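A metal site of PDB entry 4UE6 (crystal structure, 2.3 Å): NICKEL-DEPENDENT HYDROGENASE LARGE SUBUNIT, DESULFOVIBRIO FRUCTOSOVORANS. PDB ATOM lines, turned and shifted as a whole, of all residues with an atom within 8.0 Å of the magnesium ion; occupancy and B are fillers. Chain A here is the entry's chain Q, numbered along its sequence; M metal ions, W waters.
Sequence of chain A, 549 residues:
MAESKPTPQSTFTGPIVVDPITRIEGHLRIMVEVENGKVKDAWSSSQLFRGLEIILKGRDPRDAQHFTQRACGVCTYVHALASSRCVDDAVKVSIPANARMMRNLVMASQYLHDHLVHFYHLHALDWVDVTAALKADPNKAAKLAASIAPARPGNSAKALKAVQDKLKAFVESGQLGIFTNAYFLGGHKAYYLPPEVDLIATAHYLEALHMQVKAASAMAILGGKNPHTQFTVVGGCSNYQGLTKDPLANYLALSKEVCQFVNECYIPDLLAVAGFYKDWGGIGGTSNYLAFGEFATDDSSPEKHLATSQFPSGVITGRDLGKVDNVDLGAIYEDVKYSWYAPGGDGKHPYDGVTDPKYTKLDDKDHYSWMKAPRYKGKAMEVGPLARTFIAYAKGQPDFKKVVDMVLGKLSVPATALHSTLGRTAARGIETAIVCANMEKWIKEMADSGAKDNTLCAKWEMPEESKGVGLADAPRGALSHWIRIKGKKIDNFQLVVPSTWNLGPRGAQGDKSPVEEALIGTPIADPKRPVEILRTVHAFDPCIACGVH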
ATOM      1  N   PHE A  49      -0.754   3.361   7.785  1.00  0.00           N
ATOM      2  CA  PHE A  49       0.092   2.202   7.521  1.00  0.00           C
ATOM      3  C   PHE A  49       0.420   2.116   6.036  1.00  0.00           C
ATOM      4  O   PHE A  49      -0.477   2.219   5.208  1.00  0.00           O
ATOM      5  CB  PHE A  49      -0.611   0.904   7.964  1.00  0.00           C
ATOM      6  CG  PHE A  49       0.245  -0.343   7.795  1.00  0.00           C
ATOM      7  CD1 PHE A  49       1.228  -0.653   8.726  1.00  0.00           C
ATOM      8  CD2 PHE A  49       0.081  -1.170   6.702  1.00  0.00           C
ATOM      9  CE1 PHE A  49       2.031  -1.768   8.560  1.00  0.00           C
ATOM     10  CE2 PHE A  49       0.886  -2.293   6.530  1.00  0.00           C
ATOM     11  CZ  PHE A  49       1.861  -2.592   7.459  1.00  0.00           C
ATOM     12  N   GLU A  53       8.060  -3.081   5.044  1.00  0.00           N
ATOM     13  CA  GLU A  53       8.622  -4.389   5.374  1.00  0.00           C
ATOM     14  C   GLU A  53       7.984  -5.506   4.536  1.00  0.00           C
ATOM     15  O   GLU A  53       8.692  -6.390   4.048  1.00  0.00           O
ATOM     16  CB  GLU A  53       8.529  -4.687   6.882  1.00  0.00           C
ATOM     17  CG  GLU A  53       9.362  -3.740   7.728  1.00  0.00           C
ATOM     18  CD  GLU A  53       8.830  -3.582   9.142  1.00  0.00           C
ATOM     19  OE1 GLU A  53       7.635  -3.909   9.376  1.00  0.00           O
ATOM     20  OE2 GLU A  53       9.622  -3.122  10.018  1.00  0.00           O
ATOM     21  N   GLU A 334       9.927  -6.370  19.725  1.00  0.00           N
ATOM     22  CA  GLU A 334       8.737  -5.549  19.468  1.00  0.00           C
ATOM     23  C   GLU A 334       7.475  -6.306  19.875  1.00  0.00           C
ATOM     24  O   GLU A 334       7.334  -7.473  19.571  1.00  0.00           O
ATOM     25  CB  GLU A 334       8.684  -5.143  18.008  1.00  0.00           C
ATOM     26  CG  GLU A 334       9.825  -4.240  17.572  1.00  0.00           C
ATOM     27  CD  GLU A 334       9.719  -3.764  16.131  1.00  0.00           C
ATOM     28  OE1 GLU A 334       9.936  -4.571  15.200  1.00  0.00           O
ATOM     29  OE2 GLU A 334       9.453  -2.558  15.903  1.00  0.00           O
ATOM     30  N   TYR A 341      -1.980  -5.233  14.567  1.00  0.00           N
ATOM     31  CA  TYR A 341      -1.344  -6.380  13.936  1.00  0.00           C
ATOM     32  C   TYR A 341      -2.016  -7.608  14.493  1.00  0.00           C
ATOM     33  O   TYR A 341      -2.683  -7.553  15.522  1.00  0.00           O
ATOM     34  CB  TYR A 341       0.188  -6.370  14.167  1.00  0.00           C
ATOM     35  CG  TYR A 341       0.823  -5.145  13.543  1.00  0.00           C
ATOM     36  CD1 TYR A 341       1.083  -5.087  12.165  1.00  0.00           C
ATOM     37  CD2 TYR A 341       1.100  -4.019  14.312  1.00  0.00           C
ATOM     38  CE1 TYR A 341       1.608  -3.946  11.576  1.00  0.00           C
ATOM     39  CE2 TYR A 341       1.645  -2.878  13.732  1.00  0.00           C
ATOM     40  CZ  TYR A 341       1.891  -2.847  12.369  1.00  0.00           C
ATOM     41  OH  TYR A 341       2.454  -1.699  11.805  1.00  0.00           O
ATOM     42  N   PRO A 350      13.831  -8.372  16.107  1.00  0.00           N
ATOM     43  CA  PRO A 350      13.656  -7.943  14.722  1.00  0.00           C
ATOM     44  C   PRO A 350      14.125  -8.959  13.663  1.00  0.00           C
ATOM     45  O   PRO A 350      13.574  -8.964  12.569  1.00  0.00           O
ATOM     46  CB  PRO A 350      14.472  -6.646  14.639  1.00  0.00           C
ATOM     47  CG  PRO A 350      14.426  -6.110  16.019  1.00  0.00           C
ATOM     48  CD  PRO A 350      14.436  -7.302  16.926  1.00  0.00           C
ATOM     49  N   GLY A 353      11.137 -10.652  13.038  1.00  0.00           N
ATOM     50  CA  GLY A 353       9.992  -9.766  13.034  1.00  0.00           C
ATOM     51  C   GLY A 353       8.865 -10.229  12.118  1.00  0.00           C
ATOM     52  O   GLY A 353       9.094 -10.865  11.092  1.00  0.00           O
ATOM     53  N   VAL A 354       7.638  -9.917  12.505  1.00  0.00           N
ATOM     54  CA  VAL A 354       6.471 -10.243  11.737  1.00  0.00           C
ATOM     55  C   VAL A 354       5.688  -8.952  11.568  1.00  0.00           C
ATOM     56  O   VAL A 354       5.517  -8.187  12.525  1.00  0.00           O
ATOM     57  CB  VAL A 354       5.621 -11.316  12.460  1.00  0.00           C
ATOM     58  CG1 VAL A 354       4.343 -11.615  11.675  1.00  0.00           C
ATOM     59  CG2 VAL A 354       6.410 -12.619  12.577  1.00  0.00           C
ATOM     60  N   THR A 355       5.216  -8.702  10.341  1.00  0.00           N
ATOM     61  CA  THR A 355       4.366  -7.536  10.068  1.00  0.00           C
ATOM     62  C   THR A 355       3.085  -8.008   9.367  1.00  0.00           C
ATOM     63  O   THR A 355       3.047  -8.179   8.129  1.00  0.00           O
ATOM     64  CB  THR A 355       5.125  -6.509   9.224  1.00  0.00           C
ATOM     65  OG1 THR A 355       6.355  -6.166   9.888  1.00  0.00           O
ATOM     66  CG2 THR A 355       4.287  -5.232   9.014  1.00  0.00           C
ATOM     67  N   TRP A 370      -0.806   1.915  14.589  1.00  0.00           N
ATOM     68  CA  TRP A 370      -0.081   1.187  13.577  1.00  0.00           C
ATOM     69  C   TRP A 370       1.412   1.002  13.944  1.00  0.00           C
ATOM     70  O   TRP A 370       2.128   0.220  13.294  1.00  0.00           O
ATOM     71  CB  TRP A 370      -0.225   1.895  12.239  1.00  0.00           C
ATOM     72  CG  TRP A 370      -1.553   1.668  11.598  1.00  0.00           C
ATOM     73  CD1 TRP A 370      -2.536   2.611  11.404  1.00  0.00           C
ATOM     74  CD2 TRP A 370      -2.043   0.448  11.049  1.00  0.00           C
ATOM     75  NE1 TRP A 370      -3.613   2.050  10.780  1.00  0.00           N
ATOM     76  CE2 TRP A 370      -3.346   0.728  10.540  1.00  0.00           C
ATOM     77  CE3 TRP A 370      -1.518  -0.841  10.916  1.00  0.00           C
ATOM     78  CZ2 TRP A 370      -4.137  -0.253   9.909  1.00  0.00           C
ATOM     79  CZ3 TRP A 370      -2.304  -1.821  10.321  1.00  0.00           C
ATOM     80  CH2 TRP A 370      -3.597  -1.519   9.786  1.00  0.00           C
ATOM     81  N   MET A 371       1.891   1.706  14.959  1.00  0.00           N
ATOM     82  CA  MET A 371       3.240   1.420  15.424  1.00  0.00           C
ATOM     83  C   MET A 371       3.281   0.175  16.295  1.00  0.00           C
ATOM     84  O   MET A 371       2.389  -0.068  17.107  1.00  0.00           O
ATOM     85  CB  MET A 371       3.818   2.601  16.215  1.00  0.00           C
ATOM     86  CG  MET A 371       4.169   3.792  15.366  1.00  0.00           C
ATOM     87  SD  MET A 371       5.152   4.947  16.306  1.00  0.00           S
ATOM     88  CE  MET A 371       4.832   6.456  15.400  1.00  0.00           C
ATOM     89  N   LYS A 372       4.313  -0.638  16.123  1.00  0.00           N
ATOM     90  CA  LYS A 372       4.617  -1.685  17.081  1.00  0.00           C
ATOM     91  C   LYS A 372       5.170  -1.018  18.365  1.00  0.00           C
ATOM     92  O   LYS A 372       5.423   0.166  18.369  1.00  0.00           O
ATOM     93  CB  LYS A 372       5.649  -2.641  16.500  1.00  0.00           C
ATOM     94  CG  LYS A 372       5.207  -3.302  15.205  1.00  0.00           C
ATOM     95  CD  LYS A 372       6.272  -4.231  14.690  1.00  0.00           C
ATOM     96  CE  LYS A 372       5.769  -4.984  13.480  1.00  0.00           C
ATOM     97  NZ  LYS A 372       6.864  -5.793  12.862  1.00  0.00           N
ATOM     98  N   PRO A 374       8.372  -1.221  20.569  1.00  0.00           N
ATOM     99  CA  PRO A 374       9.719  -1.756  20.792  1.00  0.00           C
ATOM    100  C   PRO A 374      10.054  -1.676  22.262  1.00  0.00           C
ATOM    101  O   PRO A 374       9.768  -0.674  22.917  1.00  0.00           O
ATOM    102  CB  PRO A 374      10.634  -0.797  19.992  1.00  0.00           C
ATOM    103  CG  PRO A 374       9.731   0.062  19.177  1.00  0.00           C
ATOM    104  CD  PRO A 374       8.432   0.115  19.939  1.00  0.00           C
ATOM    105  N   SER A 480      17.487   1.031  13.633  1.00  0.00           N
ATOM    106  CA  SER A 480      18.099  -0.224  13.201  1.00  0.00           C
ATOM    107  C   SER A 480      17.298  -0.908  12.101  1.00  0.00           C
ATOM    108  O   SER A 480      16.058  -0.927  12.125  1.00  0.00           O
ATOM    109  CB  SER A 480      18.336  -1.158  14.419  1.00  0.00           C
ATOM    110  OG  SER A 480      17.141  -1.477  15.131  1.00  0.00           O
ATOM    111  N   TRP A 482      17.120  -4.614  10.020  1.00  0.00           N
ATOM    112  CA  TRP A 482      17.503  -5.999  10.251  1.00  0.00           C
ATOM    113  C   TRP A 482      17.125  -6.806   9.049  1.00  0.00           C
ATOM    114  O   TRP A 482      15.964  -6.868   8.664  1.00  0.00           O
ATOM    115  CB  TRP A 482      16.805  -6.542  11.494  1.00  0.00           C
ATOM    116  CG  TRP A 482      16.974  -5.678  12.736  1.00  0.00           C
ATOM    117  CD1 TRP A 482      16.320  -4.491  13.011  1.00  0.00           C
ATOM    118  CD2 TRP A 482      17.811  -5.939  13.873  1.00  0.00           C
ATOM    119  NE1 TRP A 482      16.704  -4.014  14.238  1.00  0.00           N
ATOM    120  CE2 TRP A 482      17.622  -4.884  14.786  1.00  0.00           C
ATOM    121  CE3 TRP A 482      18.716  -6.971  14.197  1.00  0.00           C
ATOM    122  CZ2 TRP A 482      18.304  -4.809  16.003  1.00  0.00           C
ATOM    123  CZ3 TRP A 482      19.387  -6.907  15.405  1.00  0.00           C
ATOM    124  CH2 TRP A 482      19.168  -5.823  16.300  1.00  0.00           C
ATOM    125  N   PHE A 493      12.888  -8.401   6.355  1.00  0.00           N
ATOM    126  CA  PHE A 493      13.488  -7.102   6.533  1.00  0.00           C
ATOM    127  C   PHE A 493      12.661  -6.345   7.548  1.00  0.00           C
ATOM    128  O   PHE A 493      11.484  -6.147   7.342  1.00  0.00           O
ATOM    129  CB  PHE A 493      13.537  -6.308   5.213  1.00  0.00           C
ATOM    130  CG  PHE A 493      14.577  -5.229   5.220  1.00  0.00           C
ATOM    131  CD1 PHE A 493      14.347  -4.048   5.913  1.00  0.00           C
ATOM    132  CD2 PHE A 493      15.791  -5.398   4.567  1.00  0.00           C
ATOM    133  CE1 PHE A 493      15.310  -3.051   5.967  1.00  0.00           C
ATOM    134  CE2 PHE A 493      16.767  -4.404   4.594  1.00  0.00           C
ATOM    135  CZ  PHE A 493      16.527  -3.228   5.309  1.00  0.00           C
ATOM    136  N   GLN A 494      13.266  -5.921   8.644  1.00  0.00           N
ATOM    137  CA  GLN A 494      12.507  -5.252   9.689  1.00  0.00           C
ATOM    138  C   GLN A 494      13.147  -3.931  10.036  1.00  0.00           C
ATOM    139  O   GLN A 494      14.356  -3.853  10.148  1.00  0.00           O
ATOM    140  CB  GLN A 494      12.411  -6.134  10.915  1.00  0.00           C
ATOM    141  CG  GLN A 494      11.588  -7.391  10.685  1.00  0.00           C
ATOM    142  CD  GLN A 494      10.101  -7.109  10.634  1.00  0.00           C
ATOM    143  OE1 GLN A 494       9.598  -6.265  11.400  1.00  0.00           O
ATOM    144  NE2 GLN A 494       9.386  -7.784   9.741  1.00  0.00           N
ATOM    145  N   LEU A 495      12.337  -2.893  10.163  1.00  0.00           N
ATOM    146  CA  LEU A 495      12.814  -1.590  10.605  1.00  0.00           C
ATOM    147  C   LEU A 495      12.322  -1.408  12.022  1.00  0.00           C
ATOM    148  O   LEU A 495      11.134  -1.696  12.294  1.00  0.00           O
ATOM    149  CB  LEU A 495      12.266  -0.461   9.727  1.00  0.00           C
ATOM    150  CG  LEU A 495      12.792  -0.248   8.319  1.00  0.00           C
ATOM    151  CD1 LEU A 495      12.330  -1.329   7.383  1.00  0.00           C
ATOM    152  CD2 LEU A 495      12.284   1.083   7.783  1.00  0.00           C
ATOM    153  N   VAL A 496      13.229  -0.937  12.898  1.00  0.00           N
ATOM    154  CA  VAL A 496      12.875  -0.490  14.248  1.00  0.00           C
ATOM    155  C   VAL A 496      13.396   0.943  14.342  1.00  0.00           C
ATOM    156  O   VAL A 496      14.595   1.196  14.325  1.00  0.00           O
ATOM    157  CB  VAL A 496      13.470  -1.379  15.364  1.00  0.00           C
ATOM    158  CG1 VAL A 496      12.919  -0.989  16.725  1.00  0.00           C
ATOM    159  CG2 VAL A 496      13.151  -2.847  15.106  1.00  0.00           C
ATOM    160  N   VAL A 497      12.462   1.890  14.400  1.00  0.00           N
ATOM    161  CA  VAL A 497      12.766   3.277  14.135  1.00  0.00           C
ATOM    162  C   VAL A 497      12.620   4.115  15.436  1.00  0.00           C
ATOM    163  O   VAL A 497      11.838   3.751  16.310  1.00  0.00           O
ATOM    164  CB  VAL A 497      11.899   3.773  12.955  1.00  0.00           C
ATOM    165  CG1 VAL A 497      12.326   5.152  12.468  1.00  0.00           C
ATOM    166  CG2 VAL A 497      12.058   2.820  11.791  1.00  0.00           C
ATOM    167  N   THR A 500       9.276   4.837  16.604  1.00  0.00           N
ATOM    168  CA  THR A 500       8.623   3.615  17.106  1.00  0.00           C
ATOM    169  C   THR A 500       8.932   3.438  18.589  1.00  0.00           C
ATOM    170  O   THR A 500       8.037   3.140  19.352  1.00  0.00           O
ATOM    171  CB  THR A 500       9.066   2.336  16.378  1.00  0.00           C
ATOM    172  OG1 THR A 500       9.290   2.611  14.997  1.00  0.00           O
ATOM    173  CG2 THR A 500       8.015   1.249  16.505  1.00  0.00           C
ATOM    174  N   CYS A 546       8.056   7.341   9.671  1.00  0.00           N
ATOM    175  CA  CYS A 546       9.171   6.587  10.232  1.00  0.00           C
ATOM    176  C   CYS A 546       8.734   5.483  11.206  1.00  0.00           C
ATOM    177  O   CYS A 546       9.136   4.322  11.068  1.00  0.00           O
ATOM    178  CB  CYS A 546      10.112   7.533  10.982  1.00  0.00           C
ATOM    179  SG  CYS A 546      11.541   8.032  10.027  1.00  0.00           S
ATOM    180  N   GLY A 547       7.926   5.858  12.200  1.00  0.00           N
ATOM    181  CA  GLY A 547       7.531   4.957  13.263  1.00  0.00           C
ATOM    182  C   GLY A 547       6.805   3.735  12.753  1.00  0.00           C
ATOM    183  O   GLY A 547       7.061   2.639  13.217  1.00  0.00           O
ATOM    184  N   VAL A 548       5.911   3.940  11.798  1.00  0.00           N
ATOM    185  CA  VAL A 548       5.090   2.860  11.277  1.00  0.00           C
ATOM    186  C   VAL A 548       5.720   2.163  10.068  1.00  0.00           C
ATOM    187  O   VAL A 548       5.694   0.932   9.999  1.00  0.00           O
ATOM    188  CB  VAL A 548       3.707   3.360  10.832  1.00  0.00           C
ATOM    189  CG1 VAL A 548       2.892   2.202  10.317  1.00  0.00           C
ATOM    190  CG2 VAL A 548       2.981   4.037  11.991  1.00  0.00           C
ATOM    191  N   HIS A 549       6.304   2.936   9.148  1.00  0.00           N
ATOM    192  CA  HIS A 549       6.820   2.413   7.889  1.00  0.00           C
ATOM    193  C   HIS A 549       5.848   1.405   7.196  1.00  0.00           C
ATOM    194  O   HIS A 549       6.199   0.333   6.707  1.00  0.00           O
ATOM    195  CB  HIS A 549       8.261   1.868   8.026  1.00  0.00           C
ATOM    196  CG  HIS A 549       8.510   1.106   9.291  1.00  0.00           C
ATOM    197  ND1 HIS A 549       8.750   1.720  10.509  1.00  0.00           N
ATOM    198  CD2 HIS A 549       8.555  -0.223   9.524  1.00  0.00           C
ATOM    199  CE1 HIS A 549       8.930   0.797  11.432  1.00  0.00           C
ATOM    200  NE2 HIS A 549       8.827  -0.388  10.863  1.00  0.00           N
ATOM    201  OXT HIS A 549       4.636   1.653   7.084  1.00  0.00           O
HETATM  202 MG    MG M   1       9.221  -2.267  11.955  1.00  0.00          MG
HETATM  203  O   HOH W   1       7.221  -2.749  11.647  1.00  0.00           O
HETATM  204  O   HOH W   2       9.465  -4.070  12.905  1.00  0.00           O
HETATM  205  O   HOH W   3       8.728  -1.357  13.662  1.00  0.00           O
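Glu 334 touches the magnesium ion (OE2 to MG, 3.97 Å).
The nearest printed residue that does not touch the magnesium ion is Gln 494 (4.1 Å).
Water W3 is bound to the magnesium ion, 2.0 Å away.
The magnesium ion is bound by O of Leu 495, at 2.0 Å.
Water W2 binds the magnesium ion (2.1 Å).
The magnesium ion is bound by water W1 (2.1 Å).
OE2 of Glu 53 is bound to the magnesium ion, 2.2 Å away.
NE2 of His 549 is bound to the magnesium ion (2.2 Å).
The magnesium ion has six donor atoms within binding distance.
Water W2 lies within hydrogen-bond range of OE1 of Gln 494 (2.7 Å), NZ of Lys 372 (3.1 Å) and OE2 of Glu 334 (3.4 Å).
Water W1 lies within hydrogen-bond range of the side-chain carboxylate of Glu 53 (2.6 Å) and the side-chain amino group of Lys 372 (3.3 Å).
OE1 of Gln 494 lies close to OE2 of Glu 53, 3.4 Å away.
The backbone carbonyl oxygen of Cys 546 sits at hydrogen-bond distance from a ring nitrogen (ND1) of His 549 (2.7 Å).
The side-chain hydroxyl (OG1) of Thr 355 sits at hydrogen-bond distance from the side-chain carboxylate (OE1) of Glu 53, at 2.6 Å.
A ring nitrogen (ND1) of His 549 lies close to the backbone carbonyl oxygen (O) of Gly 547.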
